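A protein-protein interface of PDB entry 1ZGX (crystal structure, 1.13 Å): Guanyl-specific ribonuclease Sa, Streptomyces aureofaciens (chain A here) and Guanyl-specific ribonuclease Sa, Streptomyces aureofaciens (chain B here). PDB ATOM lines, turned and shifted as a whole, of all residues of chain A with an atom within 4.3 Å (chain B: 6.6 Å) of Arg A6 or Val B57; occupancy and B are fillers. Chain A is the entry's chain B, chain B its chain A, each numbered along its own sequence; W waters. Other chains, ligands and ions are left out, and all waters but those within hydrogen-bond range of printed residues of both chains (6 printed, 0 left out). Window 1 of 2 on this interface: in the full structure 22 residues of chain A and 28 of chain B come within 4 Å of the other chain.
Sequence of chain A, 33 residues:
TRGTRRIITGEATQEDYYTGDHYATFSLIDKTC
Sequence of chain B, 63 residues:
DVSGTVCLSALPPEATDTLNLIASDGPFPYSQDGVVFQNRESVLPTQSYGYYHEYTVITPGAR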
ATOM      1  N   ARG A   2       7.783 -23.870 -15.200  1.00  0.00           N
ATOM      2  CA  ARG A   2       7.958 -24.361 -13.826  1.00  0.00           C
ATOM      3  C   ARG A   2       7.987 -25.877 -13.629  1.00  0.00           C
ATOM      4  O   ARG A   2       7.874 -26.366 -12.473  1.00  0.00           O
ATOM      5  CB  ARG A   2       6.920 -23.696 -12.923  1.00  0.00           C
ATOM      6  CG  ARG A   2       5.466 -24.180 -12.994  1.00  0.00           C
ATOM      7  CD  ARG A   2       4.476 -23.167 -12.491  1.00  0.00           C
ATOM      8  NE  ARG A   2       3.066 -23.603 -12.280  1.00  0.00           N
ATOM      9  CZ  ARG A   2       2.085 -23.589 -13.238  1.00  0.00           C
ATOM     10  NH1 ARG A   2       0.839 -23.959 -12.925  1.00  0.00           N
ATOM     11  NH2 ARG A   2       2.347 -23.280 -14.509  1.00  0.00           N
ATOM     12  N   GLY A   3       8.184 -26.641 -14.715  1.00  0.00           N
ATOM     13  CA  GLY A   3       8.172 -28.094 -14.634  1.00  0.00           C
ATOM     14  C   GLY A   3       6.751 -28.674 -14.571  1.00  0.00           C
ATOM     15  O   GLY A   3       5.769 -27.889 -14.748  1.00  0.00           O
ATOM     16  N   THR A   4       6.654 -29.982 -14.347  1.00  0.00           N
ATOM     17  CA  THR A   4       5.415 -30.748 -14.575  1.00  0.00           C
ATOM     18  C   THR A   4       4.789 -31.350 -13.292  1.00  0.00           C
ATOM     19  O   THR A   4       3.815 -32.149 -13.408  1.00  0.00           O
ATOM     20  CB  THR A   4       5.691 -31.875 -15.641  1.00  0.00           C
ATOM     21  OG1 THR A   4       6.667 -32.807 -15.128  1.00  0.00           O
ATOM     22  CG2 THR A   4       6.174 -31.280 -17.006  1.00  0.00           C
ATOM     23  N   ARG A   5       5.274 -30.935 -12.089  1.00  0.00           N
ATOM     24  CA  ARG A   5       4.797 -31.511 -10.820  1.00  0.00           C
ATOM     25  C   ARG A   5       3.697 -30.602 -10.173  1.00  0.00           C
ATOM     26  O   ARG A   5       3.853 -29.353 -10.131  1.00  0.00           O
ATOM     27  CB  ARG A   5       5.976 -31.702  -9.827  1.00  0.00           C
ATOM     28  CG  ARG A   5       7.180 -32.514 -10.385  1.00  0.00           C
ATOM     29  CD  ARG A   5       8.384 -32.579  -9.478  1.00  0.00           C
ATOM     30  NE  ARG A   5       9.434 -33.455 -10.111  1.00  0.00           N
ATOM     31  CZ  ARG A   5      10.694 -33.719  -9.751  1.00  0.00           C
ATOM     32  NH1 ARG A   5      11.163 -33.117  -8.698  1.00  0.00           N
ATOM     33  NH2 ARG A   5      11.492 -34.556 -10.486  1.00  0.00           N
ATOM     34  N   ARG A   6       2.613 -31.224  -9.671  1.00  0.00           N
ATOM     35  CA  ARG A   6       1.449 -30.488  -9.080  1.00  0.00           C
ATOM     36  C   ARG A   6       0.796 -31.358  -7.982  1.00  0.00           C
ATOM     37  O   ARG A   6       0.860 -32.623  -8.004  1.00  0.00           O
ATOM     38  CB  ARG A   6       0.339 -30.143 -10.128  1.00  0.00           C
ATOM     39  CG  ARG A   6       0.784 -29.467 -11.449  1.00  0.00           C
ATOM     40  CD  ARG A   6       1.058 -27.952 -11.353  1.00  0.00           C
ATOM     41  NE  ARG A   6       1.329 -27.346 -12.703  1.00  0.00           N
ATOM     42  CZ  ARG A   6       2.554 -27.310 -13.271  1.00  0.00           C
ATOM     43  NH1 ARG A   6       3.641 -27.753 -12.643  1.00  0.00           N
ATOM     44  NH2 ARG A   6       2.672 -26.815 -14.501  1.00  0.00           N
ATOM     45  N   ILE A   7       0.073 -30.668  -7.059  1.00  0.00           N
ATOM     46  CA  ILE A   7      -0.938 -31.301  -6.160  1.00  0.00           C
ATOM     47  C   ILE A   7      -2.345 -30.729  -6.502  1.00  0.00           C
ATOM     48  O   ILE A   7      -2.519 -29.495  -6.656  1.00  0.00           O
ATOM     49  CB  ILE A   7      -0.569 -31.122  -4.614  1.00  0.00           C
ATOM     50  CG1 ILE A   7       0.672 -31.983  -4.285  1.00  0.00           C
ATOM     51  CG2 ILE A   7      -1.787 -31.456  -3.670  1.00  0.00           C
ATOM     52  CD1 ILE A   7       1.214 -31.767  -2.851  1.00  0.00           C
ATOM     53  N   TYR A  17      -4.163 -35.360  -4.209  1.00  0.00           N
ATOM     54  CA  TYR A  17      -3.623 -36.169  -5.329  1.00  0.00           C
ATOM     55  C   TYR A  17      -2.299 -35.546  -5.833  1.00  0.00           C
ATOM     56  O   TYR A  17      -2.206 -34.297  -5.978  1.00  0.00           O
ATOM     57  CB  TYR A  17      -4.638 -36.251  -6.514  1.00  0.00           C
ATOM     58  CG  TYR A  17      -6.058 -36.743  -6.155  1.00  0.00           C
ATOM     59  CD1 TYR A  17      -6.414 -38.112  -6.182  1.00  0.00           C
ATOM     60  CD2 TYR A  17      -7.044 -35.825  -5.731  1.00  0.00           C
ATOM     61  CE1 TYR A  17      -7.696 -38.543  -5.843  1.00  0.00           C
ATOM     62  CE2 TYR A  17      -8.340 -36.254  -5.377  1.00  0.00           C
ATOM     63  CZ  TYR A  17      -8.669 -37.637  -5.440  1.00  0.00           C
ATOM     64  OH  TYR A  17      -9.952 -38.098  -5.057  1.00  0.00           O
ATOM     65  N   TYR A  18      -1.309 -36.412  -6.146  1.00  0.00           N
ATOM     66  CA  TYR A  18      -0.012 -35.968  -6.728  1.00  0.00           C
ATOM     67  C   TYR A  18       0.030 -36.367  -8.238  1.00  0.00           C
ATOM     68  O   TYR A  18      -0.361 -37.530  -8.630  1.00  0.00           O
ATOM     69  CB  TYR A  18       1.222 -36.621  -6.037  1.00  0.00           C
ATOM     70  CG  TYR A  18       2.573 -36.184  -6.624  1.00  0.00           C
ATOM     71  CD1 TYR A  18       3.156 -34.958  -6.214  1.00  0.00           C
ATOM     72  CD2 TYR A  18       3.292 -36.984  -7.532  1.00  0.00           C
ATOM     73  CE1 TYR A  18       4.388 -34.543  -6.694  1.00  0.00           C
ATOM     74  CE2 TYR A  18       4.545 -36.570  -8.042  1.00  0.00           C
ATOM     75  CZ  TYR A  18       5.079 -35.354  -7.625  1.00  0.00           C
ATOM     76  OH  TYR A  18       6.328 -34.899  -8.073  1.00  0.00           O
ATOM     77  N   THR A  19       0.577 -35.443  -9.076  1.00  0.00           N
ATOM     78  CA  THR A  19       0.946 -35.733 -10.485  1.00  0.00           C
ATOM     79  C   THR A  19       2.397 -35.260 -10.741  1.00  0.00           C
ATOM     80  O   THR A  19       2.790 -34.144 -10.354  1.00  0.00           O
ATOM     81  CB  THR A  19      -0.059 -35.110 -11.530  1.00  0.00           C
ATOM     82  OG1 THR A  19       0.384 -35.391 -12.898  1.00  0.00           O
ATOM     83  CG2 THR A  19      -0.179 -33.562 -11.390  1.00  0.00           C
ATOM     84  N   HIS A  22       2.041 -33.324 -15.451  1.00  0.00           N
ATOM     85  CA  HIS A  22       1.084 -32.281 -15.904  1.00  0.00           C
ATOM     86  C   HIS A  22      -0.328 -32.871 -16.124  1.00  0.00           C
ATOM     87  O   HIS A  22      -0.988 -32.611 -17.162  1.00  0.00           O
ATOM     88  CB  HIS A  22       1.594 -31.463 -17.134  1.00  0.00           C
ATOM     89  CG  HIS A  22       0.720 -30.283 -17.535  1.00  0.00           C
ATOM     90  ND1 HIS A  22      -0.003 -30.234 -18.708  1.00  0.00           N
ATOM     91  CD2 HIS A  22       0.448 -29.091 -16.888  1.00  0.00           C
ATOM     92  CE1 HIS A  22      -0.663 -29.083 -18.778  1.00  0.00           C
ATOM     93  NE2 HIS A  22      -0.412 -28.354 -17.682  1.00  0.00           N
ATOM     94  N   TYR A  23      -0.792 -33.643 -15.108  1.00  0.00           N
ATOM     95  CA  TYR A  23      -2.223 -34.106 -15.007  1.00  0.00           C
ATOM     96  C   TYR A  23      -2.540 -35.334 -15.900  1.00  0.00           C
ATOM     97  O   TYR A  23      -3.721 -35.737 -15.971  1.00  0.00           O
ATOM     98  CB  TYR A  23      -3.300 -32.974 -15.269  1.00  0.00           C
ATOM     99  CG  TYR A  23      -2.956 -31.588 -14.600  1.00  0.00           C
ATOM    100  CD1 TYR A  23      -2.888 -31.435 -13.196  1.00  0.00           C
ATOM    101  CD2 TYR A  23      -2.774 -30.448 -15.398  1.00  0.00           C
ATOM    102  CE1 TYR A  23      -2.599 -30.183 -12.619  1.00  0.00           C
ATOM    103  CE2 TYR A  23      -2.513 -29.174 -14.846  1.00  0.00           C
ATOM    104  CZ  TYR A  23      -2.415 -29.062 -13.452  1.00  0.00           C
ATOM    105  OH  TYR A  23      -2.146 -27.831 -12.843  1.00  0.00           O
ATOM    106  N   PRO B  12       9.019 -36.070  -3.821  1.00  0.00           N
ATOM    107  CA  PRO B  12      10.080 -35.051  -3.545  1.00  0.00           C
ATOM    108  C   PRO B  12       9.836 -34.253  -2.247  1.00  0.00           C
ATOM    109  O   PRO B  12       8.631 -34.048  -1.917  1.00  0.00           O
ATOM    110  CB  PRO B  12      10.062 -34.144  -4.847  1.00  0.00           C
ATOM    111  CG  PRO B  12       9.413 -34.988  -5.922  1.00  0.00           C
ATOM    112  CD  PRO B  12       8.398 -35.839  -5.157  1.00  0.00           C
ATOM    113  N   PRO B  13      10.881 -33.791  -1.535  1.00  0.00           N
ATOM    114  CA  PRO B  13      10.634 -32.998  -0.306  1.00  0.00           C
ATOM    115  C   PRO B  13       9.808 -31.704  -0.595  1.00  0.00           C
ATOM    116  O   PRO B  13       9.106 -31.181   0.319  1.00  0.00           O
ATOM    117  CB  PRO B  13      12.050 -32.778   0.251  1.00  0.00           C
ATOM    118  CG  PRO B  13      12.952 -32.883  -0.981  1.00  0.00           C
ATOM    119  CD  PRO B  13      12.357 -33.965  -1.810  1.00  0.00           C
ATOM    120  N   GLU B  14       9.877 -31.177  -1.827  1.00  0.00           N
ATOM    121  CA  GLU B  14       9.096 -29.984  -2.217  1.00  0.00           C
ATOM    122  C   GLU B  14       7.544 -30.223  -2.102  1.00  0.00           C
ATOM    123  O   GLU B  14       6.780 -29.235  -1.944  1.00  0.00           O
ATOM    124  CB  GLU B  14       9.484 -29.498  -3.631  1.00  0.00           C
ATOM    125  CG  GLU B  14      10.923 -28.960  -3.720  1.00  0.00           C
ATOM    126  CD  GLU B  14      12.029 -30.024  -3.830  1.00  0.00           C
ATOM    127  OE1 GLU B  14      11.799 -31.198  -4.135  1.00  0.00           O
ATOM    128  OE2 GLU B  14      13.234 -29.676  -3.519  1.00  0.00           O
ATOM    129  N   ALA B  15       7.099 -31.490  -2.186  1.00  0.00           N
ATOM    130  CA  ALA B  15       5.658 -31.790  -1.996  1.00  0.00           C
ATOM    131  C   ALA B  15       5.205 -31.446  -0.558  1.00  0.00           C
ATOM    132  O   ALA B  15       4.046 -31.005  -0.362  1.00  0.00           O
ATOM    133  CB  ALA B  15       5.359 -33.304  -2.356  1.00  0.00           C
ATOM    134  N   THR B  16       6.083 -31.687   0.459  1.00  0.00           N
ATOM    135  CA  THR B  16       5.758 -31.319   1.851  1.00  0.00           C
ATOM    136  C   THR B  16       5.649 -29.772   1.986  1.00  0.00           C
ATOM    137  O   THR B  16       4.743 -29.244   2.701  1.00  0.00           O
ATOM    138  CB  THR B  16       6.750 -31.891   2.889  1.00  0.00           C
ATOM    139  OG1 THR B  16       8.084 -31.247   2.747  1.00  0.00           O
ATOM    140  CG2 THR B  16       6.609 -33.499   2.873  1.00  0.00           C
ATOM    141  N   THR B  18       4.595 -27.672  -0.411  1.00  0.00           N
ATOM    142  CA  THR B  18       3.291 -27.331  -1.011  1.00  0.00           C
ATOM    143  C   THR B  18       2.126 -27.605  -0.006  1.00  0.00           C
ATOM    144  O   THR B  18       1.226 -26.741   0.141  1.00  0.00           O
ATOM    145  CB  THR B  18       3.106 -28.057  -2.377  1.00  0.00           C
ATOM    146  OG1 THR B  18       4.213 -27.737  -3.256  1.00  0.00           O
ATOM    147  CG2 THR B  18       1.765 -27.692  -3.071  1.00  0.00           C
ATOM    148  N   ASP B  33      -1.333 -20.807  -8.663  1.00  0.00           N
ATOM    149  CA  ASP B  33      -1.594 -21.534  -7.405  1.00  0.00           C
ATOM    150  C   ASP B  33      -2.923 -21.058  -6.758  1.00  0.00           C
ATOM    151  O   ASP B  33      -3.107 -19.834  -6.512  1.00  0.00           O
ATOM    152  CB  ASP B  33      -0.389 -21.383  -6.427  1.00  0.00           C
ATOM    153  CG  ASP B  33       0.917 -22.017  -6.901  1.00  0.00           C
ATOM    154  OD1 ASP B  33       0.859 -22.885  -7.877  1.00  0.00           O
ATOM    155  OD2 ASP B  33       2.014 -21.686  -6.302  1.00  0.00           O
ATOM    156  N   GLU B  54      -5.770 -26.437  -7.895  1.00  0.00           N
ATOM    157  CA  GLU B  54      -4.402 -26.820  -8.309  1.00  0.00           C
ATOM    158  C   GLU B  54      -3.295 -25.952  -7.642  1.00  0.00           C
ATOM    159  O   GLU B  54      -3.452 -24.723  -7.472  1.00  0.00           O
ATOM    160  CB  GLU B  54      -4.214 -26.757  -9.866  1.00  0.00           C
ATOM    161  CG  GLU B  54      -4.513 -25.385 -10.475  1.00  0.00           C
ATOM    162  CD  GLU B  54      -4.268 -25.382 -11.988  1.00  0.00           C
ATOM    163  OE1 GLU B  54      -3.194 -24.742 -12.382  1.00  0.00           O
ATOM    164  OE2 GLU B  54      -5.038 -26.012 -12.758  1.00  0.00           O
ATOM    165  N   TYR B  55      -2.129 -26.620  -7.361  1.00  0.00           N
ATOM    166  CA  TYR B  55      -0.963 -25.981  -6.694  1.00  0.00           C
ATOM    167  C   TYR B  55       0.364 -26.561  -7.288  1.00  0.00           C
ATOM    168  O   TYR B  55       0.505 -27.806  -7.464  1.00  0.00           O
ATOM    169  CB  TYR B  55      -0.983 -26.228  -5.141  1.00  0.00           C
ATOM    170  CG  TYR B  55      -2.280 -25.728  -4.488  1.00  0.00           C
ATOM    171  CD1 TYR B  55      -3.446 -26.554  -4.419  1.00  0.00           C
ATOM    172  CD2 TYR B  55      -2.369 -24.426  -3.985  1.00  0.00           C
ATOM    173  CE1 TYR B  55      -4.662 -26.057  -3.886  1.00  0.00           C
ATOM    174  CE2 TYR B  55      -3.578 -23.930  -3.445  1.00  0.00           C
ATOM    175  CZ  TYR B  55      -4.715 -24.750  -3.417  1.00  0.00           C
ATOM    176  OH  TYR B  55      -5.937 -24.280  -2.888  1.00  0.00           O
ATOM    177  N   THR B  56       1.359 -25.691  -7.497  1.00  0.00           N
ATOM    178  CA  THR B  56       2.672 -26.119  -8.016  1.00  0.00           C
ATOM    179  C   THR B  56       3.467 -26.874  -6.931  1.00  0.00           C
ATOM    180  O   THR B  56       3.533 -26.414  -5.753  1.00  0.00           O
ATOM    181  CB  THR B  56       3.517 -24.872  -8.498  1.00  0.00           C
ATOM    182  OG1 THR B  56       2.767 -24.085  -9.431  1.00  0.00           O
ATOM    183  CG2 THR B  56       4.862 -25.317  -9.166  1.00  0.00           C
ATOM    184  N   VAL B  57       4.139 -27.992  -7.311  1.00  0.00           N
ATOM    185  CA  VAL B  57       5.280 -28.588  -6.558  1.00  0.00           C
ATOM    186  C   VAL B  57       6.570 -28.126  -7.282  1.00  0.00           C
ATOM    187  O   VAL B  57       6.783 -28.495  -8.465  1.00  0.00           O
ATOM    188  CB  VAL B  57       5.181 -30.122  -6.434  1.00  0.00           C
ATOM    189  CG1 VAL B  57       6.407 -30.731  -5.756  1.00  0.00           C
ATOM    190  CG2 VAL B  57       3.870 -30.546  -5.664  1.00  0.00           C
ATOM    191  N   ILE B  58       7.431 -27.306  -6.617  1.00  0.00           N
ATOM    192  CA  ILE B  58       8.620 -26.781  -7.303  1.00  0.00           C
ATOM    193  C   ILE B  58       9.526 -27.952  -7.767  1.00  0.00           C
ATOM    194  O   ILE B  58       9.786 -28.909  -7.008  1.00  0.00           O
ATOM    195  CB  ILE B  58       9.377 -25.743  -6.375  1.00  0.00           C
ATOM    196  CG1 ILE B  58       8.565 -24.412  -6.324  1.00  0.00           C
ATOM    197  CG2 ILE B  58      10.847 -25.513  -6.839  1.00  0.00           C
ATOM    198  CD1 ILE B  58       9.052 -23.381  -5.330  1.00  0.00           C
ATOM    199  N   THR B  59      10.064 -27.810  -9.013  1.00  0.00           N
ATOM    200  CA  THR B  59      11.185 -28.686  -9.494  1.00  0.00           C
ATOM    201  C   THR B  59      12.471 -27.850  -9.369  1.00  0.00           C
ATOM    202  O   THR B  59      12.567 -26.774 -10.020  1.00  0.00           O
ATOM    203  CB  THR B  59      10.968 -29.115 -10.991  1.00  0.00           C
ATOM    204  OG1 THR B  59       9.774 -29.926 -11.127  1.00  0.00           O
ATOM    205  CG2 THR B  59      12.135 -29.944 -11.571  1.00  0.00           C
HETATM  206  O   HOH W   1       7.224 -28.675 -11.242  1.00  0.00           O
HETATM  207  O   HOH W   2      -0.569 -24.258 -10.203  1.00  0.00           O
HETATM  208  O   HOH W   3       9.257 -31.227 -13.596  1.00  0.00           O
HETATM  209  O   HOH W   4      13.258 -32.754  -6.043  1.00  0.00           O
HETATM  210  O   HOH W   5       9.280 -25.272 -10.283  1.00  0.00           O
HETATM  211  O   HOH W   6      10.115 -31.478  -6.641  1.00  0.00           O
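The backbone NH (N) of Val B57 sits at hydrogen-bond distance from the backbone carbonyl oxygen (O) of Arg A5, 3.1 Å away. The side-chain carboxylate (OE1) of Glu B54 sits at hydrogen-bond distance from the side-chain hydroxyl (OH) of Tyr A23, at 3.3 Å. N of Ile A7 is in hydrogen-bond range of O of Tyr B55 (2.9 Å). NE of Arg A2 sits at hydrogen-bond distance from OG1 of Thr B56.
The side-chain hydroxyl of Thr A19 is in hydrogen-bond range of the backbone NH of Tyr A23 (3.1 Å). O of Thr A19 sits at hydrogen-bond distance from N of Arg A6, 3.0 Å away. O of Thr B56 is in hydrogen-bond range of OG1 of Thr B18. OG1 of Thr B56 sits at hydrogen-bond distance from OD1 of Asp B33. The backbone carbonyl oxygen (O) of Gly A3 sits at hydrogen-bond distance from the guanidinium group (NH1) of Arg A6.
Among the printed residues, merely in contact across the chains: Arg A6 with Tyr B55, Arg A5 with Thr B59, Ile A7 with Glu B54, Tyr A18 with Pro B12, Ile A7 with Val B57, Arg A5 with Pro B12, Ile A7 with Ala B15 and Arg A6 with Val B57.
Arg A6 touches just these residues of chain B: Tyr B55 and Val B57. Printed residues of chain B within 4 Å of Ile A7: Ala B15, Glu B54, Tyr B55 and Val B57. Printed residues of chain A within 4 Å of Glu B54: Ile A7 (3.7 Å) and Tyr A23 (3.3 Å). Of the printed residues of chain B, Arg A2 touches Thr B56. Pro B13 touches none of the printed residues of chain A. Thr B18 touches none of the printed residues of chain A.
Of the 13 printed residues of chain B, 7 touch a printed residue of chain A. Printed residues of chain A that touch a printed residue of chain B: Arg A2, Arg A5, Arg A6, Ile A7, Tyr A18 and Tyr A23. Hydrophobic or aromatic side chains of chain A within 4 Å of the printed part of chain B: Ile A7, Tyr A18 and Tyr A23.
Water W6 lies within hydrogen-bond range of the backbone carbonyl oxygen (O) of Ile B58, the guanidinium group (NH1) of Arg A5 and the side-chain carboxylate (OE1) of Glu B14. Water W1 lies within hydrogen-bond range of the backbone carbonyl oxygen (O) of Arg A2 (2.7 Å), the backbone carbonyl oxygen (O) of Val B57 (2.8 Å), the side-chain hydroxyl (OG1) of Thr B59 (2.8 Å), the backbone NH (N) of Arg A5 (3.1 Å) and the backbone NH (N) of Thr A4 (3.4 Å). Water W5 lies within hydrogen-bond range of the backbone carbonyl oxygen (O) of Arg A2 (2.8 Å) and the backbone NH (N) of Thr B59 (2.9 Å). Water W3 lies within hydrogen-bond range of OG1 of Thr B59 (2.8 Å) and N of Thr A4 (3.0 Å). Water W4 lies within hydrogen-bond range of the side-chain carboxylate (OE1) of Glu B14 and the guanidinium group (NH1) of Arg A5. Water W2 lies within hydrogen-bond range of OD1 of Asp B33, NH1 of Arg A2, OG1 of Thr B56 and OE1 of Glu B54.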
